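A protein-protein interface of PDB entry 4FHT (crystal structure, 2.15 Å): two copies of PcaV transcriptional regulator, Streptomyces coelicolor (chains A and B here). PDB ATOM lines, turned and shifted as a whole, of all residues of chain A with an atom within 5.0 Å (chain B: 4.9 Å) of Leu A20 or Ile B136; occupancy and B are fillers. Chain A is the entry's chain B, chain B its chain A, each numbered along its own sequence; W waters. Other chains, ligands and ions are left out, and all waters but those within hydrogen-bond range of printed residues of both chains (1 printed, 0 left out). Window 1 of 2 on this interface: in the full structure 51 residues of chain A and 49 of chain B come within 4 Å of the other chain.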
ATOM      1  N   LEU A  16       4.227 -28.254  12.969  1.00  0.00           N
ATOM      2  CA  LEU A  16       3.180 -28.351  13.977  1.00  0.00           C
ATOM      3  C   LEU A  16       3.760 -28.184  15.377  1.00  0.00           C
ATOM      4  O   LEU A  16       3.127 -27.588  16.250  1.00  0.00           O
ATOM      5  CB  LEU A  16       2.447 -29.684  13.841  1.00  0.00           C
ATOM      6  CG  LEU A  16       1.774 -29.860  12.477  1.00  0.00           C
ATOM      7  CD1 LEU A  16       1.366 -31.305  12.242  1.00  0.00           C
ATOM      8  CD2 LEU A  16       0.570 -28.941  12.357  1.00  0.00           C
ATOM      9  N   ALA A  17       4.972 -28.696  15.577  1.00  0.00           N
ATOM     10  CA  ALA A  17       5.674 -28.534  16.847  1.00  0.00           C
ATOM     11  C   ALA A  17       5.914 -27.062  17.175  1.00  0.00           C
ATOM     12  O   ALA A  17       5.661 -26.619  18.299  1.00  0.00           O
ATOM     13  CB  ALA A  17       6.996 -29.285  16.824  1.00  0.00           C
ATOM     14  N   ARG A  18       6.414 -26.311  16.198  1.00  0.00           N
ATOM     15  CA  ARG A  18       6.668 -24.889  16.394  1.00  0.00           C
ATOM     16  C   ARG A  18       5.389 -24.132  16.746  1.00  0.00           C
ATOM     17  O   ARG A  18       5.374 -23.326  17.675  1.00  0.00           O
ATOM     18  CB  ARG A  18       7.319 -24.261  15.158  1.00  0.00           C
ATOM     19  CG  ARG A  18       7.368 -22.740  15.247  1.00  0.00           C
ATOM     20  CD  ARG A  18       8.063 -22.084  14.074  1.00  0.00           C
ATOM     21  NE  ARG A  18       7.335 -22.217  12.812  1.00  0.00           N
ATOM     22  CZ  ARG A  18       6.242 -21.529  12.490  1.00  0.00           C
ATOM     23  NH1 ARG A  18       5.710 -20.669  13.348  1.00  0.00           N
ATOM     24  NH2 ARG A  18       5.671 -21.710  11.308  1.00  0.00           N
ATOM     25  N   ARG A  19       4.320 -24.398  16.001  1.00  0.00           N
ATOM     26  CA  ARG A  19       3.028 -23.760  16.248  1.00  0.00           C
ATOM     27  C   ARG A  19       2.489 -24.064  17.640  1.00  0.00           C
ATOM     28  O   ARG A  19       1.979 -23.178  18.322  1.00  0.00           O
ATOM     29  CB  ARG A  19       1.996 -24.208  15.208  1.00  0.00           C
ATOM     30  CG  ARG A  19       2.067 -23.498  13.866  1.00  0.00           C
ATOM     31  CD  ARG A  19       0.948 -24.017  12.971  1.00  0.00           C
ATOM     32  NE  ARG A  19       0.885 -23.353  11.674  1.00  0.00           N
ATOM     33  CZ  ARG A  19       0.076 -22.336  11.390  1.00  0.00           C
ATOM     34  NH1 ARG A  19      -0.739 -21.851  12.318  1.00  0.00           N
ATOM     35  NH2 ARG A  19       0.084 -21.804  10.176  1.00  0.00           N
ATOM     36  N   LEU A  20       2.588 -25.324  18.051  1.00  0.00           N
ATOM     37  CA  LEU A  20       2.047 -25.750  19.336  1.00  0.00           C
ATOM     38  C   LEU A  20       2.772 -25.057  20.481  1.00  0.00           C
ATOM     39  O   LEU A  20       2.147 -24.581  21.430  1.00  0.00           O
ATOM     40  CB  LEU A  20       2.155 -27.268  19.488  1.00  0.00           C
ATOM     41  CG  LEU A  20       1.648 -27.861  20.802  1.00  0.00           C
ATOM     42  CD1 LEU A  20       0.137 -27.717  20.912  1.00  0.00           C
ATOM     43  CD2 LEU A  20       2.061 -29.317  20.936  1.00  0.00           C
ATOM     44  N   GLN A  21       4.095 -24.993  20.374  1.00  0.00           N
ATOM     45  CA  GLN A  21       4.918 -24.360  21.395  1.00  0.00           C
ATOM     46  C   GLN A  21       4.705 -22.853  21.409  1.00  0.00           C
ATOM     47  O   GLN A  21       4.755 -22.225  22.467  1.00  0.00           O
ATOM     48  CB  GLN A  21       6.403 -24.701  21.198  1.00  0.00           C
ATOM     49  CG  GLN A  21       7.358 -23.953  22.132  1.00  0.00           C
ATOM     50  CD  GLN A  21       7.056 -24.170  23.613  1.00  0.00           C
ATOM     51  OE1 GLN A  21       6.339 -25.095  23.990  1.00  0.00           O
ATOM     52  NE2 GLN A  21       7.613 -23.310  24.459  1.00  0.00           N
ATOM     53  N   GLN A  22       4.465 -22.280  20.231  1.00  0.00           N
ATOM     54  CA  GLN A  22       4.080 -20.876  20.129  1.00  0.00           C
ATOM     55  C   GLN A  22       2.771 -20.647  20.869  1.00  0.00           C
ATOM     56  O   GLN A  22       2.632 -19.683  21.616  1.00  0.00           O
ATOM     57  CB  GLN A  22       3.918 -20.453  18.667  1.00  0.00           C
ATOM     58  CG  GLN A  22       5.211 -20.093  17.962  1.00  0.00           C
ATOM     59  CD  GLN A  22       4.979 -19.603  16.543  1.00  0.00           C
ATOM     60  OE1 GLN A  22       5.927 -19.344  15.802  1.00  0.00           O
ATOM     61  NE2 GLN A  22       3.714 -19.474  16.158  1.00  0.00           N
ATOM     62  N   ALA A  23       1.809 -21.536  20.643  1.00  0.00           N
ATOM     63  CA  ALA A  23       0.523 -21.463  21.323  1.00  0.00           C
ATOM     64  C   ALA A  23       0.709 -21.606  22.831  1.00  0.00           C
ATOM     65  O   ALA A  23       0.098 -20.878  23.614  1.00  0.00           O
ATOM     66  CB  ALA A  23      -0.420 -22.538  20.795  1.00  0.00           C
ATOM     67  N   HIS A  24       1.561 -22.548  23.224  1.00  0.00           N
ATOM     68  CA  HIS A  24       1.890 -22.769  24.629  1.00  0.00           C
ATOM     69  C   HIS A  24       2.455 -21.505  25.269  1.00  0.00           C
ATOM     70  O   HIS A  24       2.000 -21.075  26.329  1.00  0.00           O
ATOM     71  CB  HIS A  24       2.912 -23.904  24.747  1.00  0.00           C
ATOM     72  CG  HIS A  24       3.425 -24.119  26.138  1.00  0.00           C
ATOM     73  ND1 HIS A  24       4.697 -24.582  26.396  1.00  0.00           N
ATOM     74  CD2 HIS A  24       2.834 -23.952  27.345  1.00  0.00           C
ATOM     75  CE1 HIS A  24       4.873 -24.681  27.702  1.00  0.00           C
ATOM     76  NE2 HIS A  24       3.755 -24.307  28.301  1.00  0.00           N
ATOM     77  N   PHE A 120      -6.357 -25.008  26.825  1.00  0.00           N
ATOM     78  CA  PHE A 120      -5.421 -25.611  25.882  1.00  0.00           C
ATOM     79  C   PHE A 120      -5.959 -26.915  25.292  1.00  0.00           C
ATOM     80  O   PHE A 120      -5.801 -27.176  24.098  1.00  0.00           O
ATOM     81  CB  PHE A 120      -4.068 -25.858  26.561  1.00  0.00           C
ATOM     82  CG  PHE A 120      -2.885 -25.755  25.632  1.00  0.00           C
ATOM     83  CD1 PHE A 120      -3.062 -25.625  24.266  1.00  0.00           C
ATOM     84  CD2 PHE A 120      -1.591 -25.792  26.132  1.00  0.00           C
ATOM     85  CE1 PHE A 120      -1.973 -25.531  23.415  1.00  0.00           C
ATOM     86  CE2 PHE A 120      -0.500 -25.701  25.288  1.00  0.00           C
ATOM     87  CZ  PHE A 120      -0.692 -25.571  23.925  1.00  0.00           C
ATOM     88  N   PHE A 132      -3.522 -37.903  22.423  1.00  0.00           N
ATOM     89  CA  PHE A 132      -2.632 -36.772  22.182  1.00  0.00           C
ATOM     90  C   PHE A 132      -1.357 -36.860  23.018  1.00  0.00           C
ATOM     91  O   PHE A 132      -0.259 -36.745  22.481  1.00  0.00           O
ATOM     92  CB  PHE A 132      -3.352 -35.449  22.449  1.00  0.00           C
ATOM     93  CG  PHE A 132      -2.451 -34.245  22.400  1.00  0.00           C
ATOM     94  CD1 PHE A 132      -1.897 -33.825  21.203  1.00  0.00           C
ATOM     95  CD2 PHE A 132      -2.167 -33.529  23.552  1.00  0.00           C
ATOM     96  CE1 PHE A 132      -1.069 -32.716  21.154  1.00  0.00           C
ATOM     97  CE2 PHE A 132      -1.341 -32.416  23.513  1.00  0.00           C
ATOM     98  CZ  PHE A 132      -0.793 -32.009  22.313  1.00  0.00           C
ATOM     99  N   ILE A 136       2.335 -37.572  21.154  1.00  0.00           N
ATOM    100  CA  ILE A 136       3.312 -36.491  21.202  1.00  0.00           C
ATOM    101  C   ILE A 136       4.546 -36.878  22.015  1.00  0.00           C
ATOM    102  O   ILE A 136       5.655 -36.446  21.712  1.00  0.00           O
ATOM    103  CB  ILE A 136       2.696 -35.177  21.737  1.00  0.00           C
ATOM    104  CG1 ILE A 136       3.634 -34.000  21.467  1.00  0.00           C
ATOM    105  CG2 ILE A 136       2.379 -35.278  23.223  1.00  0.00           C
ATOM    106  CD1 ILE A 136       3.039 -32.660  21.833  1.00  0.00           C
ATOM    107  N   ALA B  17       4.639 -29.955  24.794  1.00  0.00           N
ATOM    108  CA  ALA B  17       4.870 -29.020  23.700  1.00  0.00           C
ATOM    109  C   ALA B  17       6.315 -28.537  23.670  1.00  0.00           C
ATOM    110  O   ALA B  17       6.944 -28.508  22.610  1.00  0.00           O
ATOM    111  CB  ALA B  17       3.922 -27.836  23.800  1.00  0.00           C
ATOM    112  N   LEU B  20       8.651 -31.407  22.627  1.00  0.00           N
ATOM    113  CA  LEU B  20       8.516 -31.702  21.205  1.00  0.00           C
ATOM    114  C   LEU B  20       9.281 -30.684  20.362  1.00  0.00           C
ATOM    115  O   LEU B  20       9.948 -31.044  19.391  1.00  0.00           O
ATOM    116  CB  LEU B  20       7.043 -31.724  20.793  1.00  0.00           C
ATOM    117  CG  LEU B  20       6.771 -32.004  19.313  1.00  0.00           C
ATOM    118  CD1 LEU B  20       7.242 -33.397  18.924  1.00  0.00           C
ATOM    119  CD2 LEU B  20       5.296 -31.820  18.987  1.00  0.00           C
ATOM    120  N   VAL B 131      -3.652 -39.190  12.742  1.00  0.00           N
ATOM    121  CA  VAL B 131      -4.279 -38.754  13.983  1.00  0.00           C
ATOM    122  C   VAL B 131      -3.422 -37.699  14.676  1.00  0.00           C
ATOM    123  O   VAL B 131      -3.933 -36.678  15.141  1.00  0.00           O
ATOM    124  CB  VAL B 131      -4.504 -39.938  14.942  1.00  0.00           C
ATOM    125  CG1 VAL B 131      -4.980 -39.443  16.302  1.00  0.00           C
ATOM    126  CG2 VAL B 131      -5.506 -40.920  14.346  1.00  0.00           C
ATOM    127  N   PHE B 132      -2.118 -37.950  14.732  1.00  0.00           N
ATOM    128  CA  PHE B 132      -1.178 -37.024  15.356  1.00  0.00           C
ATOM    129  C   PHE B 132      -1.253 -35.640  14.722  1.00  0.00           C
ATOM    130  O   PHE B 132      -1.352 -34.637  15.427  1.00  0.00           O
ATOM    131  CB  PHE B 132       0.251 -37.568  15.272  1.00  0.00           C
ATOM    132  CG  PHE B 132       1.301 -36.602  15.746  1.00  0.00           C
ATOM    133  CD1 PHE B 132       1.483 -36.363  17.097  1.00  0.00           C
ATOM    134  CD2 PHE B 132       2.111 -35.939  14.837  1.00  0.00           C
ATOM    135  CE1 PHE B 132       2.452 -35.478  17.535  1.00  0.00           C
ATOM    136  CE2 PHE B 132       3.082 -35.053  15.271  1.00  0.00           C
ATOM    137  CZ  PHE B 132       3.253 -34.824  16.621  1.00  0.00           C
ATOM    138  N   PHE B 133      -1.212 -35.595  13.392  1.00  0.00           N
ATOM    139  CA  PHE B 133      -1.319 -34.337  12.662  1.00  0.00           C
ATOM    140  C   PHE B 133      -2.608 -33.605  13.018  1.00  0.00           C
ATOM    141  O   PHE B 133      -2.597 -32.399  13.274  1.00  0.00           O
ATOM    142  CB  PHE B 133      -1.264 -34.575  11.149  1.00  0.00           C
ATOM    143  CG  PHE B 133       0.068 -35.065  10.655  1.00  0.00           C
ATOM    144  CD1 PHE B 133       1.241 -34.667  11.273  1.00  0.00           C
ATOM    145  CD2 PHE B 133       0.145 -35.927   9.573  1.00  0.00           C
ATOM    146  CE1 PHE B 133       2.468 -35.118  10.819  1.00  0.00           C
ATOM    147  CE2 PHE B 133       1.369 -36.383   9.117  1.00  0.00           C
ATOM    148  CZ  PHE B 133       2.531 -35.978   9.742  1.00  0.00           C
ATOM    149  N   ASP B 134      -3.715 -34.340  13.039  1.00  0.00           N
ATOM    150  CA  ASP B 134      -5.017 -33.740  13.317  1.00  0.00           C
ATOM    151  C   ASP B 134      -5.121 -33.184  14.737  1.00  0.00           C
ATOM    152  O   ASP B 134      -5.582 -32.061  14.938  1.00  0.00           O
ATOM    153  CB  ASP B 134      -6.141 -34.744  13.061  1.00  0.00           C
ATOM    154  CG  ASP B 134      -7.512 -34.167  13.356  1.00  0.00           C
ATOM    155  OD1 ASP B 134      -7.970 -33.300  12.581  1.00  0.00           O
ATOM    156  OD2 ASP B 134      -8.130 -34.579  14.362  1.00  0.00           O
ATOM    157  N   LEU B 135      -4.689 -33.971  15.717  1.00  0.00           N
ATOM    158  CA  LEU B 135      -4.805 -33.564  17.114  1.00  0.00           C
ATOM    159  C   LEU B 135      -3.944 -32.347  17.439  1.00  0.00           C
ATOM    160  O   LEU B 135      -4.419 -31.395  18.051  1.00  0.00           O
ATOM    161  CB  LEU B 135      -4.464 -34.725  18.053  1.00  0.00           C
ATOM    162  CG  LEU B 135      -5.345 -35.975  17.957  1.00  0.00           C
ATOM    163  CD1 LEU B 135      -5.025 -36.942  19.091  1.00  0.00           C
ATOM    164  CD2 LEU B 135      -6.826 -35.614  17.948  1.00  0.00           C
ATOM    165  N   ILE B 136      -2.681 -32.377  17.024  1.00  0.00           N
ATOM    166  CA  ILE B 136      -1.756 -31.301  17.356  1.00  0.00           C
ATOM    167  C   ILE B 136      -2.146 -29.970  16.710  1.00  0.00           C
ATOM    168  O   ILE B 136      -1.997 -28.913  17.322  1.00  0.00           O
ATOM    169  CB  ILE B 136      -0.284 -31.663  17.026  1.00  0.00           C
ATOM    170  CG1 ILE B 136       0.667 -30.625  17.622  1.00  0.00           C
ATOM    171  CG2 ILE B 136      -0.064 -31.787  15.528  1.00  0.00           C
ATOM    172  CD1 ILE B 136       2.126 -30.972  17.443  1.00  0.00           C
ATOM    173  N   ARG B 137      -2.661 -30.022  15.486  1.00  0.00           N
ATOM    174  CA  ARG B 137      -3.107 -28.811  14.809  1.00  0.00           C
ATOM    175  C   ARG B 137      -4.285 -28.196  15.555  1.00  0.00           C
ATOM    176  O   ARG B 137      -4.344 -26.982  15.753  1.00  0.00           O
ATOM    177  CB  ARG B 137      -3.502 -29.107  13.362  1.00  0.00           C
ATOM    178  CG  ARG B 137      -4.085 -27.907  12.632  1.00  0.00           C
ATOM    179  CD  ARG B 137      -4.634 -28.295  11.269  1.00  0.00           C
ATOM    180  NE  ARG B 137      -5.570 -29.412  11.364  1.00  0.00           N
ATOM    181  CZ  ARG B 137      -6.866 -29.284  11.626  1.00  0.00           C
ATOM    182  NH1 ARG B 137      -7.391 -28.081  11.822  1.00  0.00           N
ATOM    183  NH2 ARG B 137      -7.637 -30.360  11.693  1.00  0.00           N
ATOM    184  N   ARG B 138      -5.215 -29.048  15.974  1.00  0.00           N
ATOM    185  CA  ARG B 138      -6.380 -28.602  16.731  1.00  0.00           C
ATOM    186  C   ARG B 138      -5.974 -27.995  18.074  1.00  0.00           C
ATOM    187  O   ARG B 138      -6.477 -26.943  18.461  1.00  0.00           O
ATOM    188  CB  ARG B 138      -7.370 -29.754  16.922  1.00  0.00           C
ATOM    189  CG  ARG B 138      -8.109 -30.142  15.648  1.00  0.00           C
ATOM    190  CD  ARG B 138      -8.740 -31.523  15.758  1.00  0.00           C
ATOM    191  NE  ARG B 138      -9.640 -31.628  16.902  1.00  0.00           N
ATOM    192  CZ  ARG B 138     -10.179 -32.767  17.324  1.00  0.00           C
ATOM    193  NH1 ARG B 138      -9.906 -33.902  16.695  1.00  0.00           N
ATOM    194  NH2 ARG B 138     -10.985 -32.772  18.376  1.00  0.00           N
ATOM    195  N   VAL B 139      -5.051 -28.647  18.771  1.00  0.00           N
ATOM    196  CA  VAL B 139      -4.570 -28.131  20.050  1.00  0.00           C
ATOM    197  C   VAL B 139      -3.781 -26.836  19.864  1.00  0.00           C
ATOM    198  O   VAL B 139      -3.856 -25.928  20.693  1.00  0.00           O
ATOM    199  CB  VAL B 139      -3.706 -29.171  20.797  1.00  0.00           C
ATOM    200  CG1 VAL B 139      -3.178 -28.595  22.104  1.00  0.00           C
ATOM    201  CG2 VAL B 139      -4.512 -30.423  21.068  1.00  0.00           C
ATOM    202  N   ALA B 140      -3.040 -26.743  18.764  1.00  0.00           N
ATOM    203  CA  ALA B 140      -2.257 -25.541  18.481  1.00  0.00           C
ATOM    204  C   ALA B 140      -3.150 -24.330  18.220  1.00  0.00           C
ATOM    205  O   ALA B 140      -2.743 -23.191  18.440  1.00  0.00           O
ATOM    206  CB  ALA B 140      -1.311 -25.776  17.311  1.00  0.00           C
HETATM  207  O   HOH W   1       5.651 -28.494  20.386  1.00  0.00           O
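Water W1 lies within hydrogen-bond range of O of Ala B17 (2.6 Å) and O of Ala A17 (2.8 Å).
The side-chain amide oxygen (OE1) of Gln A21 lies within hydrogen-bond range of a ring nitrogen (ND1) of His A24, at 3.0 Å.
Leu A16 touches Phe B133.
Ala A17 touches Leu B20.
Ala B17 touches Leu A20.
Leu A20 touches Val B139 (CD1 to CG1, 3.6 Å).
Gln A21 touches Ala B17 (OE1 to C, 3.5 Å).
Ala B140 touches Ala A23.
Val B139 touches Phe A120.
Phe A132 touches Leu B135 (N to CD1, 3.8 Å).
Ile A136 touches Leu B20 (CG1 to CD2, 3.7 Å).
Phe B132 touches Ile A136 (CE1 to CA, 3.9 Å).
Of the 12 printed residues of chain A, 8 touch a printed residue of chain B.
Hydrophobic or aromatic side chains of chain A that line the printed part of chain B: Leu A16, Ala A17, Leu A20, Ala A23, Phe A120 and Ile A136.
Of the 12 printed residues of chain B, 8 touch a printed residue of chain A.
Printed residues of chain B that touch a printed residue of chain A: Ala B17, Leu B20, Phe B132, Phe B133, Leu B135, Ile B136, Val B139 and Ala B140.
Along chain B the printed residues that touch a printed residue of chain A span positions 17 to 140.
Ala A17 touches Leu B20, and with the chains exchanged Leu A20 touches Ala B17.
Leu A20 touches Ile B136, and with the chains exchanged Ile A136 touches Leu B20.
Ile A136 touches Phe B132, but with the chains exchanged Phe A132 does not touch Ile B136 (4.1 Å).
Of chain B, only Ala B17 (3.7 Å), Ile B136 (3.8 Å), Val B139 (3.6 Å) and Ala B140 (3.9 Å) come within 4 Å of Leu A20.
Of the printed residues of chain B, Ile A136 touches Leu B20 (3.7 Å) and Phe B132 (3.9 Å).
Of the printed residues of chain A, Leu B20 touches Ala A17 and Ile A136.
Ile B136 touches just these residues of chain A: Leu A16 (3.6 Å) and Leu A20 (3.8 Å).
Printed residues of chain A within 4 Å of Ala B140: Leu A20 (3.9 Å) and Ala A23 (3.4 Å).
The nearest printed residue of chain A that does not touch Ile B136 is Ala A17 (4.1 Å).
The nearest printed residue of chain A that does not touch Ala B140 is Arg A19 (4.2 Å).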
